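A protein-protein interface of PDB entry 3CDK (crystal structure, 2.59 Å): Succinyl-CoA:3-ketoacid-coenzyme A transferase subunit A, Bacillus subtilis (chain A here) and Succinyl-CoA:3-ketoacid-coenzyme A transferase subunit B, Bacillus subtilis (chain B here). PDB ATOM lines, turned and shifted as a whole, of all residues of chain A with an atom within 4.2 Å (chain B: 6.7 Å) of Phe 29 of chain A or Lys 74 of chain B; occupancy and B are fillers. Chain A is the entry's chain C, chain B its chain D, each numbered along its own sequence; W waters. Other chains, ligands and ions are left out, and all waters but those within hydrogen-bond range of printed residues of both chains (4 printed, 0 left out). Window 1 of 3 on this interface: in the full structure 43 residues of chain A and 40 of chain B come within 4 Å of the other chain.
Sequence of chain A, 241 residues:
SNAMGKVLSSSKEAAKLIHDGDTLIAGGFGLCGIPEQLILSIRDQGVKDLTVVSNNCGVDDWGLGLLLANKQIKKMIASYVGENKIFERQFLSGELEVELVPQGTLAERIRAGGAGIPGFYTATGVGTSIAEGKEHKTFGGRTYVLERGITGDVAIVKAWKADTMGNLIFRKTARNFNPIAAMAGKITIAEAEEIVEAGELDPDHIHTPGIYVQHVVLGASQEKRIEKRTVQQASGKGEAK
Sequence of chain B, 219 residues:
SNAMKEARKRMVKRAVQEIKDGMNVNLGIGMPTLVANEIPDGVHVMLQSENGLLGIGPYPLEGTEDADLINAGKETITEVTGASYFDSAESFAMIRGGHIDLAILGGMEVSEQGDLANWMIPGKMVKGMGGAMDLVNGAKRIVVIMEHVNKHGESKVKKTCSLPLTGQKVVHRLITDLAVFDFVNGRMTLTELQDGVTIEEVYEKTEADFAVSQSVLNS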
ATOM      1  N   GLY A  28      31.795   9.602  34.914  1.00  0.00           N
ATOM      2  CA  GLY A  28      30.472  10.213  34.829  1.00  0.00           C
ATOM      3  C   GLY A  28      30.452  11.134  33.620  1.00  0.00           C
ATOM      4  O   GLY A  28      31.476  11.739  33.281  1.00  0.00           O
ATOM      5  N   PHE A  29      29.308  11.223  32.955  1.00  0.00           N
ATOM      6  CA  PHE A  29      29.073  12.200  31.905  1.00  0.00           C
ATOM      7  C   PHE A  29      27.823  12.976  32.304  1.00  0.00           C
ATOM      8  O   PHE A  29      26.719  12.408  32.335  1.00  0.00           O
ATOM      9  CB  PHE A  29      28.812  11.459  30.623  1.00  0.00           C
ATOM     10  CG  PHE A  29      28.549  12.327  29.433  1.00  0.00           C
ATOM     11  CD1 PHE A  29      29.596  12.763  28.640  1.00  0.00           C
ATOM     12  CD2 PHE A  29      27.244  12.620  29.050  1.00  0.00           C
ATOM     13  CE1 PHE A  29      29.368  13.541  27.512  1.00  0.00           C
ATOM     14  CE2 PHE A  29      26.983  13.388  27.913  1.00  0.00           C
ATOM     15  CZ  PHE A  29      28.053  13.855  27.138  1.00  0.00           C
ATOM     16  N   GLY A  30      27.992  14.273  32.583  1.00  0.00           N
ATOM     17  CA  GLY A  30      26.935  15.093  33.151  1.00  0.00           C
ATOM     18  C   GLY A  30      26.574  14.502  34.499  1.00  0.00           C
ATOM     19  O   GLY A  30      27.411  14.409  35.389  1.00  0.00           O
ATOM     20  N   LEU A  31      25.333  14.075  34.663  1.00  0.00           N
ATOM     21  CA  LEU A  31      24.968  13.489  35.936  1.00  0.00           C
ATOM     22  C   LEU A  31      24.797  11.981  35.799  1.00  0.00           C
ATOM     23  O   LEU A  31      24.276  11.317  36.685  1.00  0.00           O
ATOM     24  CB  LEU A  31      23.720  14.166  36.515  1.00  0.00           C
ATOM     25  CG  LEU A  31      23.791  15.587  37.122  1.00  0.00           C
ATOM     26  CD1 LEU A  31      22.450  15.910  37.824  1.00  0.00           C
ATOM     27  CD2 LEU A  31      24.955  15.755  38.082  1.00  0.00           C
ATOM     28  N   CYS A  32      25.301  11.453  34.691  1.00  0.00           N
ATOM     29  CA  CYS A  32      25.112  10.072  34.338  1.00  0.00           C
ATOM     30  C   CYS A  32      26.320   9.176  34.644  1.00  0.00           C
ATOM     31  O   CYS A  32      27.411   9.411  34.130  1.00  0.00           O
ATOM     32  CB  CYS A  32      24.742  10.015  32.872  1.00  0.00           C
ATOM     33  SG  CYS A  32      24.133   8.441  32.413  1.00  0.00           S
ATOM     34  N   ASN A  55      35.106  14.544  32.738  1.00  0.00           N
ATOM     35  CA  ASN A  55      34.536  15.207  31.548  1.00  0.00           C
ATOM     36  C   ASN A  55      33.897  16.546  31.862  1.00  0.00           C
ATOM     37  O   ASN A  55      34.166  17.551  31.186  1.00  0.00           O
ATOM     38  CB  ASN A  55      33.484  14.324  30.858  1.00  0.00           C
ATOM     39  CG  ASN A  55      33.002  14.919  29.534  1.00  0.00           C
ATOM     40  OD1 ASN A  55      31.804  15.220  29.364  1.00  0.00           O
ATOM     41  ND2 ASN A  55      33.942  15.127  28.594  1.00  0.00           N
ATOM     42  N   ASN A  56      33.036  16.553  32.876  1.00  0.00           N
ATOM     43  CA  ASN A  56      32.375  17.776  33.286  1.00  0.00           C
ATOM     44  C   ASN A  56      32.579  17.927  34.746  1.00  0.00           C
ATOM     45  O   ASN A  56      33.181  17.052  35.379  1.00  0.00           O
ATOM     46  CB  ASN A  56      30.869  17.686  33.059  1.00  0.00           C
ATOM     47  CG  ASN A  56      30.516  17.041  31.763  1.00  0.00           C
ATOM     48  OD1 ASN A  56      30.416  15.816  31.671  1.00  0.00           O
ATOM     49  ND2 ASN A  56      30.309  17.854  30.749  1.00  0.00           N
ATOM     50  N   GLN A 103      37.023  16.318  24.213  1.00  0.00           N
ATOM     51  CA  GLN A 103      36.517  15.147  24.908  1.00  0.00           C
ATOM     52  C   GLN A 103      37.262  13.895  24.434  1.00  0.00           C
ATOM     53  O   GLN A 103      37.702  13.048  25.249  1.00  0.00           O
ATOM     54  CB  GLN A 103      35.008  15.062  24.728  1.00  0.00           C
ATOM     55  CG  GLN A 103      34.353  13.954  25.494  1.00  0.00           C
ATOM     56  CD  GLN A 103      32.811  14.063  25.587  1.00  0.00           C
ATOM     57  OE1 GLN A 103      32.254  15.110  25.892  1.00  0.00           O
ATOM     58  NE2 GLN A 103      32.145  12.954  25.392  1.00  0.00           N
ATOM     59  N   ASN A 176      30.366   5.550  30.034  1.00  0.00           N
ATOM     60  CA  ASN A 176      31.196   6.675  29.617  1.00  0.00           C
ATOM     61  C   ASN A 176      32.675   6.577  30.045  1.00  0.00           C
ATOM     62  O   ASN A 176      33.413   5.718  29.560  1.00  0.00           O
ATOM     63  CB  ASN A 176      30.539   8.015  30.042  1.00  0.00           C
ATOM     64  CG  ASN A 176      30.202   8.085  31.553  1.00  0.00           C
ATOM     65  OD1 ASN A 176      31.087   8.363  32.386  1.00  0.00           O
ATOM     66  ND2 ASN A 176      28.934   7.862  31.897  1.00  0.00           N
ATOM     67  N   GLU A 227      19.167  15.530  34.482  1.00  0.00           N
ATOM     68  CA  GLU A 227      19.305  16.947  34.200  1.00  0.00           C
ATOM     69  C   GLU A 227      18.142  17.432  33.357  1.00  0.00           C
ATOM     70  O   GLU A 227      17.446  18.382  33.738  1.00  0.00           O
ATOM     71  CB  GLU A 227      20.626  17.229  33.491  1.00  0.00           C
ATOM     72  CG  GLU A 227      20.874  18.709  33.239  1.00  0.00           C
ATOM     73  CD  GLU A 227      22.315  19.010  32.864  1.00  0.00           C
ATOM     74  OE1 GLU A 227      23.223  18.250  33.290  1.00  0.00           O
ATOM     75  OE2 GLU A 227      22.529  20.016  32.143  1.00  0.00           O
ATOM     76  N   LYS A 228      17.931  16.768  32.215  1.00  0.00           N
ATOM     77  CA  LYS A 228      16.774  17.059  31.376  1.00  0.00           C
ATOM     78  C   LYS A 228      15.830  15.852  31.278  1.00  0.00           C
ATOM     79  O   LYS A 228      16.191  14.821  30.726  1.00  0.00           O
ATOM     80  CB  LYS A 228      17.225  17.532  29.992  1.00  0.00           C
ATOM     81  CG  LYS A 228      18.186  18.752  30.041  1.00  0.00           C
ATOM     82  CD  LYS A 228      18.242  19.418  28.654  1.00  0.00           C
ATOM     83  CE  LYS A 228      19.519  20.227  28.480  1.00  0.00           C
ATOM     84  NZ  LYS A 228      20.087  20.069  27.105  1.00  0.00           N
ATOM     85  N   ILE B  29      24.901  18.961  19.860  1.00  0.00           N
ATOM     86  CA  ILE B  29      23.895  19.548  20.786  1.00  0.00           C
ATOM     87  C   ILE B  29      23.290  20.810  20.170  1.00  0.00           C
ATOM     88  O   ILE B  29      23.941  21.492  19.373  1.00  0.00           O
ATOM     89  CB  ILE B  29      24.432  19.812  22.253  1.00  0.00           C
ATOM     90  CG1 ILE B  29      23.446  20.638  23.119  1.00  0.00           C
ATOM     91  CG2 ILE B  29      25.712  20.593  22.230  1.00  0.00           C
ATOM     92  CD1 ILE B  29      22.047  19.981  23.487  1.00  0.00           C
ATOM     93  N   SER B  49      25.749   8.822  19.923  1.00  0.00           N
ATOM     94  CA  SER B  49      25.944   9.752  21.020  1.00  0.00           C
ATOM     95  C   SER B  49      27.375   9.587  21.558  1.00  0.00           C
ATOM     96  O   SER B  49      27.747   8.496  21.985  1.00  0.00           O
ATOM     97  CB  SER B  49      24.914   9.496  22.124  1.00  0.00           C
ATOM     98  OG  SER B  49      24.624  10.691  22.827  1.00  0.00           O
ATOM     99  N   GLU B  50      28.151  10.673  21.555  1.00  0.00           N
ATOM    100  CA  GLU B  50      29.567  10.631  21.973  1.00  0.00           C
ATOM    101  C   GLU B  50      29.820  10.209  23.412  1.00  0.00           C
ATOM    102  O   GLU B  50      30.966   9.960  23.788  1.00  0.00           O
ATOM    103  CB  GLU B  50      30.331  11.938  21.675  1.00  0.00           C
ATOM    104  CG  GLU B  50      29.769  13.193  22.286  1.00  0.00           C
ATOM    105  CD  GLU B  50      28.862  13.950  21.306  1.00  0.00           C
ATOM    106  OE1 GLU B  50      27.899  13.340  20.698  1.00  0.00           O
ATOM    107  OE2 GLU B  50      29.126  15.178  21.163  1.00  0.00           O
ATOM    108  N   ASN B  51      28.758  10.135  24.211  1.00  0.00           N
ATOM    109  CA  ASN B  51      28.864   9.577  25.558  1.00  0.00           C
ATOM    110  C   ASN B  51      28.840   8.034  25.616  1.00  0.00           C
ATOM    111  O   ASN B  51      28.945   7.449  26.689  1.00  0.00           O
ATOM    112  CB  ASN B  51      27.861  10.227  26.525  1.00  0.00           C
ATOM    113  CG  ASN B  51      26.420  10.203  26.020  1.00  0.00           C
ATOM    114  OD1 ASN B  51      25.488  10.179  26.817  1.00  0.00           O
ATOM    115  ND2 ASN B  51      26.233  10.219  24.714  1.00  0.00           N
ATOM    116  N   ILE B  70      21.021   8.703  28.413  1.00  0.00           N
ATOM    117  CA  ILE B  70      20.889  10.122  28.022  1.00  0.00           C
ATOM    118  C   ILE B  70      21.687  10.409  26.760  1.00  0.00           C
ATOM    119  O   ILE B  70      22.537   9.586  26.357  1.00  0.00           O
ATOM    120  CB  ILE B  70      21.347  11.118  29.140  1.00  0.00           C
ATOM    121  CG1 ILE B  70      22.837  10.920  29.466  1.00  0.00           C
ATOM    122  CG2 ILE B  70      20.467  10.999  30.381  1.00  0.00           C
ATOM    123  CD1 ILE B  70      23.372  11.848  30.562  1.00  0.00           C
ATOM    124  N   ASN B  71      21.404  11.555  26.130  1.00  0.00           N
ATOM    125  CA  ASN B  71      22.215  12.007  25.003  1.00  0.00           C
ATOM    126  C   ASN B  71      23.357  12.918  25.498  1.00  0.00           C
ATOM    127  O   ASN B  71      23.425  13.244  26.673  1.00  0.00           O
ATOM    128  CB  ASN B  71      21.352  12.714  23.967  1.00  0.00           C
ATOM    129  CG  ASN B  71      20.776  14.020  24.487  1.00  0.00           C
ATOM    130  OD1 ASN B  71      21.282  14.604  25.460  1.00  0.00           O
ATOM    131  ND2 ASN B  71      19.695  14.478  23.857  1.00  0.00           N
ATOM    132  N   ALA B  72      24.236  13.351  24.601  1.00  0.00           N
ATOM    133  CA  ALA B  72      25.329  14.209  25.018  1.00  0.00           C
ATOM    134  C   ALA B  72      24.850  15.522  25.589  1.00  0.00           C
ATOM    135  O   ALA B  72      25.587  16.155  26.342  1.00  0.00           O
ATOM    136  CB  ALA B  72      26.299  14.448  23.890  1.00  0.00           C
ATOM    137  N   GLY B  73      23.626  15.939  25.243  1.00  0.00           N
ATOM    138  CA  GLY B  73      23.052  17.183  25.787  1.00  0.00           C
ATOM    139  C   GLY B  73      22.398  17.007  27.153  1.00  0.00           C
ATOM    140  O   GLY B  73      21.799  17.956  27.699  1.00  0.00           O
ATOM    141  N   LYS B  74      22.500  15.794  27.705  1.00  0.00           N
ATOM    142  CA  LYS B  74      21.991  15.495  29.046  1.00  0.00           C
ATOM    143  C   LYS B  74      20.466  15.233  29.083  1.00  0.00           C
ATOM    144  O   LYS B  74      19.889  15.013  30.154  1.00  0.00           O
ATOM    145  CB  LYS B  74      22.381  16.607  30.035  1.00  0.00           C
ATOM    146  CG  LYS B  74      23.805  16.525  30.629  1.00  0.00           C
ATOM    147  CD  LYS B  74      24.894  16.338  29.585  1.00  0.00           C
ATOM    148  CE  LYS B  74      25.992  17.357  29.716  1.00  0.00           C
ATOM    149  NZ  LYS B  74      27.203  16.978  28.896  1.00  0.00           N
ATOM    150  N   GLU B  75      19.835  15.234  27.907  1.00  0.00           N
ATOM    151  CA  GLU B  75      18.435  14.843  27.768  1.00  0.00           C
ATOM    152  C   GLU B  75      18.201  13.332  27.804  1.00  0.00           C
ATOM    153  O   GLU B  75      18.866  12.550  27.136  1.00  0.00           O
ATOM    154  CB  GLU B  75      17.853  15.347  26.462  1.00  0.00           C
ATOM    155  CG  GLU B  75      18.044  16.789  26.197  1.00  0.00           C
ATOM    156  CD  GLU B  75      17.774  17.100  24.753  1.00  0.00           C
ATOM    157  OE1 GLU B  75      18.365  16.415  23.893  1.00  0.00           O
ATOM    158  OE2 GLU B  75      16.981  18.024  24.478  1.00  0.00           O
ATOM    159  N   THR B  76      17.212  12.956  28.588  1.00  0.00           N
ATOM    160  CA  THR B  76      16.751  11.596  28.721  1.00  0.00           C
ATOM    161  C   THR B  76      16.264  11.109  27.340  1.00  0.00           C
ATOM    162  O   THR B  76      15.553  11.836  26.658  1.00  0.00           O
ATOM    163  CB  THR B  76      15.656  11.602  29.849  1.00  0.00           C
ATOM    164  OG1 THR B  76      15.866  10.519  30.760  1.00  0.00           O
ATOM    165  CG2 THR B  76      14.259  11.612  29.327  1.00  0.00           C
ATOM    166  N   SER B  88      33.910   5.834  26.687  1.00  0.00           N
ATOM    167  CA  SER B  88      34.361   7.077  26.095  1.00  0.00           C
ATOM    168  C   SER B  88      35.600   6.943  25.208  1.00  0.00           C
ATOM    169  O   SER B  88      35.580   7.419  24.064  1.00  0.00           O
ATOM    170  CB  SER B  88      34.549   8.143  27.161  1.00  0.00           C
ATOM    171  OG  SER B  88      33.289   8.481  27.721  1.00  0.00           O
HETATM  172  O   HOH W   1      29.780  17.194  27.410  1.00  0.00           O
HETATM  173  O   HOH W   2      32.301  10.300  26.042  1.00  0.00           O
HETATM  174  O   HOH W   3      28.786   4.783  27.811  1.00  0.00           O
HETATM  175  O   HOH W   4      26.058   9.198  29.936  1.00  0.00           O
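The backbone NH of Lys 228 of chain A is in hydrogen-bond range of the backbone carbonyl oxygen of Lys 74 of chain B, 3.3 Å away.
O of Gly 73 of chain B lies within hydrogen-bond range of NZ of Lys 228 of chain A, 2.8 Å away.
O of Lys 228 of chain A sits at hydrogen-bond distance from N of Thr 76 of chain B (3.0 Å).
O of Asn 176 of chain A is in hydrogen-bond range of N of Ser 88 of chain B.
The backbone NH (N) of Phe 29 of chain A sits at hydrogen-bond distance from the side-chain amide oxygen (OD1) of Asn 176 of chain A, at 3.4 Å.
N of Gly 73 of chain B lies within hydrogen-bond range of OD1 of Asn 71 of chain B, at 2.7 Å.
The side-chain amide oxygen (OD1) of Asn 55 of chain A lies close to the side-chain amide oxygen (OD1) of Asn 56 of chain A, at 2.8 Å.
OD1 of Asn 51 of chain B sits close to O of Ile 70 of chain B, 3.0 Å away.
The backbone carbonyl oxygen (O) of Ala 72 of chain B sits at hydrogen-bond distance from the side-chain amino group (NZ) of Lys 74 of chain B (3.1 Å).
The backbone carbonyl oxygen of Cys 32 of chain A is in hydrogen-bond range of the side-chain amide nitrogen of Asn 176 of chain A, at 3.1 Å.
Among the printed residues, pairs that only touch across the chains: Phe 29 of chain A with Asn 51 of chain B (3.5 Å), Phe 29 of chain A with Ile 70 of chain B (3.8 Å), Phe 29 of chain A with Asn 71 of chain B (3.8 Å), Phe 29 of chain A with Ala 72 of chain B (3.4 Å), Phe 29 of chain A with Lys 74 of chain B (3.7 Å), Cys 32 of chain A with Ile 70 of chain B (3.3 Å), Asn 56 of chain A with Lys 74 of chain B (3.7 Å), Gln 103 of chain A with Glu 50 of chain B (3.6 Å), Asn 176 of chain A with Asn 51 of chain B (3.8 Å), Glu 227 of chain A with Lys 74 of chain B (3.2 Å) and Lys 228 of chain A with Glu 75 of chain B (3.6 Å).
Of the printed residues of chain B, Phe 29 of chain A touches Asn 51, Ile 70, Asn 71, Ala 72 and Lys 74.
Printed residues of chain A within 4 Å of Lys 74 of chain B: Phe 29 (3.7 Å), Asn 56 (3.7 Å), Glu 227 (3.2 Å) and Lys 228 (3.3 Å).
Printed residues of chain B within 4 Å of Gln 103 of chain A: Glu 50.
Of the printed residues of chain A, Glu 75 of chain B touches Lys 228 (3.6 Å).
Of the printed residues of chain A, Ile 70 of chain B touches Phe 29 (3.8 Å) and Cys 32 (3.3 Å).
Of the printed residues of chain B, Lys 228 of chain A touches Gly 73 (2.8 Å), Lys 74 (3.3 Å), Glu 75 (3.6 Å) and Thr 76 (3.0 Å).
Of the printed residues of chain B, Asn 176 of chain A touches Asn 51 (3.8 Å) and Ser 88 (2.9 Å).
Asn 55 of chain A touches none of the printed residues of chain B.
The nearest residue of chain B that does not touch Phe 29 of chain A is Gly 73 of chain B (5.0 Å).
The nearest printed residue of chain A that does not touch Lys 74 of chain B is Gly 30 of chain A (4.2 Å).
The nearest printed residue of chain A that does not touch Asn 71 of chain B is Lys 228 of chain A (5.8 Å).
Printed residues of chain B that touch a printed residue of chain A: Glu 50, Asn 51, Ile 70, Asn 71, Ala 72, Gly 73, Lys 74, Glu 75, Thr 76 and Ser 88.
Of the 11 printed residues of chain A, 7 touch a printed residue of chain B.
Hydrophobic or aromatic side chains of chain A within 4 Å of the printed part of chain B: Phe 29.
Among the printed residues, 15 pairs touch across the chains.
Water W2 lies within hydrogen-bond range of O of Glu 50 of chain B (2.6 Å), OG of Ser 88 of chain B (2.7 Å) and NE2 of Gln 103 of chain A (2.7 Å).
Water W3 bridges N of Asn 176 of chain A (2.8 Å) and O of Asn 51 of chain B (2.9 Å).
Water W1 lies within hydrogen-bond range of NZ of Lys 74 of chain B, OD1 of Asn 55 of chain A and ND2 of Asn 56 of chain A.
Water W4 lies within hydrogen-bond range of SG of Cys 32 of chain A and OD1 of Asn 51 of chain B.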
